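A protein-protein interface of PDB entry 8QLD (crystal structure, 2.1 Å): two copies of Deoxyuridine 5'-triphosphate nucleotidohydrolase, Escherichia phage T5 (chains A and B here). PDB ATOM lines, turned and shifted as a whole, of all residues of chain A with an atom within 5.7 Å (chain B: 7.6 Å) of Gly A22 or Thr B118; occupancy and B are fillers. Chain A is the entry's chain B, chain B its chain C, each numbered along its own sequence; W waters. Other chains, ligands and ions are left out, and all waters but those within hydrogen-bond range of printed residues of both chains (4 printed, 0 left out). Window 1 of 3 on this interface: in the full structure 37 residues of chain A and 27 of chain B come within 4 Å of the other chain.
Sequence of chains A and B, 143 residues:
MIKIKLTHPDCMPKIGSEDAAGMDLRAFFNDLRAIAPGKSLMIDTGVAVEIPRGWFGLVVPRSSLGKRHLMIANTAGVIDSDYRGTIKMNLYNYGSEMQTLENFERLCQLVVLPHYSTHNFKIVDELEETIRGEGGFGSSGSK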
ATOM      1  N   ILE A   2      11.511   6.248 -20.291  1.00  0.00           N
ATOM      2  CA  ILE A   2      11.184   4.943 -20.857  1.00  0.00           C
ATOM      3  C   ILE A   2      11.843   3.856 -20.009  1.00  0.00           C
ATOM      4  O   ILE A   2      13.068   3.767 -19.916  1.00  0.00           O
ATOM      5  CB  ILE A   2      11.612   4.847 -22.335  1.00  0.00           C
ATOM      6  CG1 ILE A   2      10.889   5.880 -23.204  1.00  0.00           C
ATOM      7  CG2 ILE A   2      11.405   3.446 -22.869  1.00  0.00           C
ATOM      8  CD1 ILE A   2      11.719   6.404 -24.320  1.00  0.00           C
ATOM      9  N   LYS A  14      20.666   0.426 -29.670  1.00  0.00           N
ATOM     10  CA  LYS A  14      21.719   1.395 -29.901  1.00  0.00           C
ATOM     11  C   LYS A  14      21.132   2.792 -29.678  1.00  0.00           C
ATOM     12  O   LYS A  14      20.147   3.190 -30.313  1.00  0.00           O
ATOM     13  CB  LYS A  14      22.299   1.211 -31.305  1.00  0.00           C
ATOM     14  CG  LYS A  14      23.525   2.048 -31.645  1.00  0.00           C
ATOM     15  CD  LYS A  14      24.744   1.689 -30.825  1.00  0.00           C
ATOM     16  CE  LYS A  14      25.992   2.492 -31.155  1.00  0.00           C
ATOM     17  NZ  LYS A  14      26.643   2.028 -32.405  1.00  0.00           N
ATOM     18  N   ILE A  15      21.753   3.494 -28.738  1.00  0.00           N
ATOM     19  CA  ILE A  15      21.446   4.866 -28.391  1.00  0.00           C
ATOM     20  C   ILE A  15      22.421   5.775 -29.132  1.00  0.00           C
ATOM     21  O   ILE A  15      23.622   5.711 -28.901  1.00  0.00           O
ATOM     22  CB  ILE A  15      21.588   5.055 -26.872  1.00  0.00           C
ATOM     23  CG1 ILE A  15      20.776   4.014 -26.091  1.00  0.00           C
ATOM     24  CG2 ILE A  15      21.237   6.475 -26.476  1.00  0.00           C
ATOM     25  CD1 ILE A  15      19.296   4.054 -26.338  1.00  0.00           C
ATOM     26  N   GLY A  16      21.889   6.654 -29.981  1.00  0.00           N
ATOM     27  CA  GLY A  16      22.708   7.624 -30.673  1.00  0.00           C
ATOM     28  C   GLY A  16      22.953   8.843 -29.790  1.00  0.00           C
ATOM     29  O   GLY A  16      22.951   8.753 -28.562  1.00  0.00           O
ATOM     30  N   SER A  17      23.142   9.992 -30.440  1.00  0.00           N
ATOM     31  CA  SER A  17      23.401  11.224 -29.727  1.00  0.00           C
ATOM     32  C   SER A  17      22.084  11.814 -29.253  1.00  0.00           C
ATOM     33  O   SER A  17      21.012  11.290 -29.566  1.00  0.00           O
ATOM     34  CB  SER A  17      24.131  12.190 -30.593  1.00  0.00           C
ATOM     35  OG  SER A  17      23.219  12.802 -31.477  1.00  0.00           O
ATOM     36  N   ALA A  20      19.423  12.074 -31.952  1.00  0.00           N
ATOM     37  CA  ALA A  20      18.879  10.898 -32.598  1.00  0.00           C
ATOM     38  C   ALA A  20      17.376  10.863 -32.323  1.00  0.00           C
ATOM     39  O   ALA A  20      16.953  11.046 -31.183  1.00  0.00           O
ATOM     40  CB  ALA A  20      19.585   9.678 -32.074  1.00  0.00           C
ATOM     41  N   ALA A  21      16.576  10.669 -33.385  1.00  0.00           N
ATOM     42  CA  ALA A  21      15.134  10.611 -33.246  1.00  0.00           C
ATOM     43  C   ALA A  21      14.753   9.341 -32.500  1.00  0.00           C
ATOM     44  O   ALA A  21      13.816   9.332 -31.708  1.00  0.00           O
ATOM     45  CB  ALA A  21      14.476  10.659 -34.604  1.00  0.00           C
ATOM     46  N   GLY A  22      15.476   8.261 -32.774  1.00  0.00           N
ATOM     47  CA  GLY A  22      15.126   6.976 -32.204  1.00  0.00           C
ATOM     48  C   GLY A  22      16.337   6.140 -31.836  1.00  0.00           C
ATOM     49  O   GLY A  22      17.472   6.516 -32.108  1.00  0.00           O
ATOM     50  N   MET A  23      16.060   5.045 -31.147  1.00  0.00           N
ATOM     51  CA  MET A  23      17.046   4.051 -30.785  1.00  0.00           C
ATOM     52  C   MET A  23      16.871   2.819 -31.681  1.00  0.00           C
ATOM     53  O   MET A  23      15.769   2.427 -32.066  1.00  0.00           O
ATOM     54  CB  MET A  23      16.895   3.649 -29.315  1.00  0.00           C
ATOM     55  CG  MET A  23      15.547   3.068 -28.933  1.00  0.00           C
ATOM     56  SD  MET A  23      15.408   2.854 -27.105  1.00  0.00           S
ATOM     57  CE  MET A  23      15.414   4.547 -26.519  1.00  0.00           C
ATOM     58  N   ASP A  24      17.991   2.201 -32.030  1.00  0.00           N
ATOM     59  CA  ASP A  24      17.962   1.162 -33.038  1.00  0.00           C
ATOM     60  C   ASP A  24      17.632  -0.168 -32.361  1.00  0.00           C
ATOM     61  O   ASP A  24      18.416  -0.628 -31.548  1.00  0.00           O
ATOM     62  CB  ASP A  24      19.292   1.080 -33.773  1.00  0.00           C
ATOM     63  CG  ASP A  24      19.586   2.224 -34.730  1.00  0.00           C
ATOM     64  OD1 ASP A  24      18.658   2.921 -35.150  1.00  0.00           O
ATOM     65  OD2 ASP A  24      20.767   2.363 -35.076  1.00  0.00           O
ATOM     66  N   GLN A 109      14.206   1.364 -36.123  1.00  0.00           N
ATOM     67  CA  GLN A 109      14.335   2.427 -35.143  1.00  0.00           C
ATOM     68  C   GLN A 109      13.014   2.565 -34.394  1.00  0.00           C
ATOM     69  O   GLN A 109      11.940   2.470 -34.991  1.00  0.00           O
ATOM     70  CB  GLN A 109      14.794   3.737 -35.782  1.00  0.00           C
ATOM     71  CG  GLN A 109      14.078   4.167 -37.049  1.00  0.00           C
ATOM     72  CD  GLN A 109      14.983   5.069 -37.846  1.00  0.00           C
ATOM     73  OE1 GLN A 109      15.194   4.867 -39.048  1.00  0.00           O
ATOM     74  NE2 GLN A 109      15.565   6.051 -37.155  1.00  0.00           N
ATOM     75  N   LEU A 110      13.133   2.732 -33.074  1.00  0.00           N
ATOM     76  CA  LEU A 110      12.006   3.028 -32.206  1.00  0.00           C
ATOM     77  C   LEU A 110      12.044   4.514 -31.895  1.00  0.00           C
ATOM     78  O   LEU A 110      13.051   5.003 -31.379  1.00  0.00           O
ATOM     79  CB  LEU A 110      12.122   2.216 -30.921  1.00  0.00           C
ATOM     80  CG  LEU A 110      11.199   2.638 -29.779  1.00  0.00           C
ATOM     81  CD1 LEU A 110       9.737   2.441 -30.121  1.00  0.00           C
ATOM     82  CD2 LEU A 110      11.527   1.842 -28.532  1.00  0.00           C
ATOM     83  N   VAL A 111      11.016   5.232 -32.327  1.00  0.00           N
ATOM     84  CA  VAL A 111      10.899   6.658 -32.048  1.00  0.00           C
ATOM     85  C   VAL A 111       9.733   6.811 -31.082  1.00  0.00           C
ATOM     86  O   VAL A 111       8.732   6.130 -31.259  1.00  0.00           O
ATOM     87  CB  VAL A 111      10.697   7.470 -33.347  1.00  0.00           C
ATOM     88  CG1 VAL A 111      10.632   8.968 -33.071  1.00  0.00           C
ATOM     89  CG2 VAL A 111      11.771   7.160 -34.387  1.00  0.00           C
ATOM     90  N   PHE B  56      12.465  15.856 -35.268  1.00  0.00           N
ATOM     91  CA  PHE B  56      13.024  15.129 -36.395  1.00  0.00           C
ATOM     92  C   PHE B  56      12.091  15.214 -37.603  1.00  0.00           C
ATOM     93  O   PHE B  56      10.942  15.655 -37.506  1.00  0.00           O
ATOM     94  CB  PHE B  56      13.275  13.667 -36.027  1.00  0.00           C
ATOM     95  CG  PHE B  56      12.024  12.828 -36.027  1.00  0.00           C
ATOM     96  CD1 PHE B  56      11.190  12.788 -34.925  1.00  0.00           C
ATOM     97  CD2 PHE B  56      11.714  12.025 -37.114  1.00  0.00           C
ATOM     98  CE1 PHE B  56      10.069  11.973 -34.913  1.00  0.00           C
ATOM     99  CE2 PHE B  56      10.594  11.224 -37.093  1.00  0.00           C
ATOM    100  CZ  PHE B  56       9.758  11.223 -36.009  1.00  0.00           C
ATOM    101  N   VAL B  78      13.837   9.154 -41.707  1.00  0.00           N
ATOM    102  CA  VAL B  78      13.907   9.747 -40.385  1.00  0.00           C
ATOM    103  C   VAL B  78      15.106  10.683 -40.371  1.00  0.00           C
ATOM    104  O   VAL B  78      16.244  10.229 -40.347  1.00  0.00           O
ATOM    105  CB  VAL B  78      13.973   8.673 -39.275  1.00  0.00           C
ATOM    106  CG1 VAL B  78      14.050   9.288 -37.872  1.00  0.00           C
ATOM    107  CG2 VAL B  78      12.776   7.743 -39.335  1.00  0.00           C
ATOM    108  N   ASP B  80      17.407  13.122 -38.609  1.00  0.00           N
ATOM    109  CA  ASP B  80      17.810  13.547 -37.277  1.00  0.00           C
ATOM    110  C   ASP B  80      18.132  15.037 -37.275  1.00  0.00           C
ATOM    111  O   ASP B  80      18.567  15.605 -38.283  1.00  0.00           O
ATOM    112  CB  ASP B  80      19.043  12.768 -36.815  1.00  0.00           C
ATOM    113  CG  ASP B  80      18.800  11.282 -36.610  1.00  0.00           C
ATOM    114  OD1 ASP B  80      17.679  10.903 -36.312  1.00  0.00           O
ATOM    115  OD2 ASP B  80      19.761  10.511 -36.770  1.00  0.00           O
ATOM    116  N   HIS B 115      10.185  14.237 -30.628  1.00  0.00           N
ATOM    117  CA  HIS B 115      10.505  12.908 -30.138  1.00  0.00           C
ATOM    118  C   HIS B 115      11.011  12.981 -28.706  1.00  0.00           C
ATOM    119  O   HIS B 115      11.752  13.897 -28.353  1.00  0.00           O
ATOM    120  CB  HIS B 115      11.551  12.232 -31.013  1.00  0.00           C
ATOM    121  CG  HIS B 115      12.899  12.844 -30.961  1.00  0.00           C
ATOM    122  ND1 HIS B 115      13.803  12.567 -29.968  1.00  0.00           N
ATOM    123  CD2 HIS B 115      13.486  13.704 -31.777  1.00  0.00           C
ATOM    124  CE1 HIS B 115      14.920  13.261 -30.194  1.00  0.00           C
ATOM    125  NE2 HIS B 115      14.745  13.955 -31.303  1.00  0.00           N
ATOM    126  N   TYR B 116      10.658  11.951 -27.936  1.00  0.00           N
ATOM    127  CA  TYR B 116      11.217  11.741 -26.620  1.00  0.00           C
ATOM    128  C   TYR B 116      12.723  11.598 -26.762  1.00  0.00           C
ATOM    129  O   TYR B 116      13.211  11.064 -27.773  1.00  0.00           O
ATOM    130  CB  TYR B 116      10.592  10.466 -26.061  1.00  0.00           C
ATOM    131  CG  TYR B 116      10.434  10.410 -24.546  1.00  0.00           C
ATOM    132  CD1 TYR B 116       9.352  11.020 -23.929  1.00  0.00           C
ATOM    133  CD2 TYR B 116      11.327   9.704 -23.748  1.00  0.00           C
ATOM    134  CE1 TYR B 116       9.185  10.967 -22.562  1.00  0.00           C
ATOM    135  CE2 TYR B 116      11.172   9.646 -22.372  1.00  0.00           C
ATOM    136  CZ  TYR B 116      10.103  10.291 -21.781  1.00  0.00           C
ATOM    137  OH  TYR B 116       9.917  10.224 -20.443  1.00  0.00           O
ATOM    138  N   SER B 117      13.443  12.064 -25.730  1.00  0.00           N
ATOM    139  CA  SER B 117      14.896  11.913 -25.708  1.00  0.00           C
ATOM    140  C   SER B 117      15.252  10.435 -25.600  1.00  0.00           C
ATOM    141  O   SER B 117      14.745   9.739 -24.721  1.00  0.00           O
ATOM    142  CB  SER B 117      15.538  12.693 -24.580  1.00  0.00           C
ATOM    143  OG  SER B 117      16.913  12.356 -24.509  1.00  0.00           O
ATOM    144  N   THR B 118      16.116   9.956 -26.490  1.00  0.00           N
ATOM    145  CA  THR B 118      16.446   8.540 -26.513  1.00  0.00           C
ATOM    146  C   THR B 118      17.427   8.232 -25.378  1.00  0.00           C
ATOM    147  O   THR B 118      17.739   7.068 -25.125  1.00  0.00           O
ATOM    148  CB  THR B 118      17.019   8.112 -27.877  1.00  0.00           C
ATOM    149  OG1 THR B 118      18.285   8.742 -28.067  1.00  0.00           O
ATOM    150  CG2 THR B 118      16.120   8.414 -29.062  1.00  0.00           C
ATOM    151  N   HIS B 119      17.939   9.289 -24.724  1.00  0.00           N
ATOM    152  CA  HIS B 119      18.778   9.142 -23.549  1.00  0.00           C
ATOM    153  C   HIS B 119      17.905   8.950 -22.311  1.00  0.00           C
ATOM    154  O   HIS B 119      18.405   8.481 -21.304  1.00  0.00           O
ATOM    155  CB  HIS B 119      19.755  10.322 -23.399  1.00  0.00           C
ATOM    156  CG  HIS B 119      21.071  10.114 -24.083  1.00  0.00           C
ATOM    157  ND1 HIS B 119      21.441  10.743 -25.255  1.00  0.00           N
ATOM    158  CD2 HIS B 119      22.123   9.329 -23.747  1.00  0.00           C
ATOM    159  CE1 HIS B 119      22.658  10.328 -25.621  1.00  0.00           C
ATOM    160  NE2 HIS B 119      23.104   9.486 -24.711  1.00  0.00           N
ATOM    161  N   ASN B 120      16.613   9.291 -22.361  1.00  0.00           N
ATOM    162  CA  ASN B 120      15.820   9.289 -21.137  1.00  0.00           C
ATOM    163  C   ASN B 120      15.137   7.938 -20.927  1.00  0.00           C
ATOM    164  O   ASN B 120      13.932   7.788 -21.131  1.00  0.00           O
ATOM    165  CB  ASN B 120      14.786  10.412 -21.112  1.00  0.00           C
ATOM    166  CG  ASN B 120      14.114  10.506 -19.759  1.00  0.00           C
ATOM    167  OD1 ASN B 120      14.586   9.913 -18.784  1.00  0.00           O
ATOM    168  ND2 ASN B 120      13.028  11.262 -19.690  1.00  0.00           N
ATOM    169  N   PHE B 121      15.917   6.958 -20.468  1.00  0.00           N
ATOM    170  CA  PHE B 121      15.415   5.606 -20.268  1.00  0.00           C
ATOM    171  C   PHE B 121      16.089   5.042 -19.021  1.00  0.00           C
ATOM    172  O   PHE B 121      17.096   5.592 -18.604  1.00  0.00           O
ATOM    173  CB  PHE B 121      15.706   4.733 -21.500  1.00  0.00           C
ATOM    174  CG  PHE B 121      17.160   4.394 -21.651  1.00  0.00           C
ATOM    175  CD1 PHE B 121      18.029   5.256 -22.288  1.00  0.00           C
ATOM    176  CD2 PHE B 121      17.683   3.265 -21.047  1.00  0.00           C
ATOM    177  CE1 PHE B 121      19.389   4.984 -22.342  1.00  0.00           C
ATOM    178  CE2 PHE B 121      19.046   3.001 -21.080  1.00  0.00           C
ATOM    179  CZ  PHE B 121      19.897   3.856 -21.738  1.00  0.00           C
HETATM  180  O   HOH W   1      19.322   6.959 -29.687  1.00  0.00           O
HETATM  181  O   HOH W   2      12.376   9.148 -29.548  1.00  0.00           O
HETATM  182  O   HOH W   3      17.470  11.449 -28.608  1.00  0.00           O
HETATM  183  O   HOH W   4      17.417   8.610 -38.092  1.00  0.00           O
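The backbone NH (N) of Ile A2 sits at hydrogen-bond distance from the backbone carbonyl oxygen (O) of Asn B120 (3.0 Å).
N of Ala A21 lies within hydrogen-bond range of OD1 of Asp B80, at 3.1 Å.
ND2 of Asn B120 lies within hydrogen-bond range of OH of Tyr B116 (3.4 Å).
The backbone NH (N) of His B119 sits close to the side-chain hydroxyl (OG) of Ser B117 (3.2 Å).
O of Met A23 lies within hydrogen-bond range of N of Leu A110.
CD1 of Ile A2 touches CD2 of Tyr B116, at 3.4 Å.
O of Ile A2 touches CA of Phe B121, 3.0 Å away.
Ile A15 touches Thr B118.
Gly A16 touches His B119 (O to CE1, 3.3 Å).
Ala A20 touches Asp B80 (CA to OD1, 3.9 Å).
Ala A20 touches Thr B118 (O to CG2, 3.5 Å).
Phe B56 touches Ala A21 (CB to CB, 3.5 Å).
Ala A21 touches Val B78 (CB to CG1, 3.6 Å).
His B115 touches Ala A21 (ND1 to O, 3.7 Å).
Val B78 touches Gln A109 (CG1 to NE2, 3.6 Å).
Of chain B, only Thr B118 comes within 4 Å of Gly A22.
Of chain A, only Ile A15, Ala A20, Ala A21, Gly A22 and Met A23 come within 4 Å of Thr B118.
Printed residues of chain B within 4 Å of Ala A21: Phe B56 (3.5 Å), Val B78 (3.6 Å), Asp B80 (3.1 Å), His B115 (3.7 Å) and Thr B118 (3.6 Å).
Of the printed residues of chain A, Val B78 touches Ala A21 (3.6 Å) and Gln A109 (3.6 Å).
Printed residues of chain B within 4 Å of Gln A109: Val B78.
Leu A110 touches none of the printed residues of chain B.
Hydrophobic or aromatic side chains of chain B that line the printed part of chain A: Phe B56, Val B78, His B115, Tyr B116, His B119 and Phe B121.
Along chain B the printed residues that touch a printed residue of chain A span positions 56 to 121.
Of the 13 printed residues of chain A, 10 touch a printed residue of chain B.
Among the printed residues, no Asp or Glu carboxylate lies within 4 Å of a Lys or Arg side-chain nitrogen of the other chain.
No position is printed for both chains.
Water W1 lies within hydrogen-bond range of the backbone NH of Gly A16, the side-chain hydroxyl of Thr B118 and the backbone carbonyl oxygen of Gly A22.
Water W2 bridges the backbone carbonyl oxygen (O) of Ala A21 (2.6 Å) and the backbone carbonyl oxygen (O) of Tyr B116 (2.7 Å).
Water W3 lies within hydrogen-bond range of O of Ala A20 (2.7 Å) and OG1 of Thr B118 (2.9 Å).
Water W4 lies within hydrogen-bond range of OD1 of Asp B80 (2.9 Å), O of Val B78 (3.0 Å) and NE2 of Gln A109 (3.3 Å).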
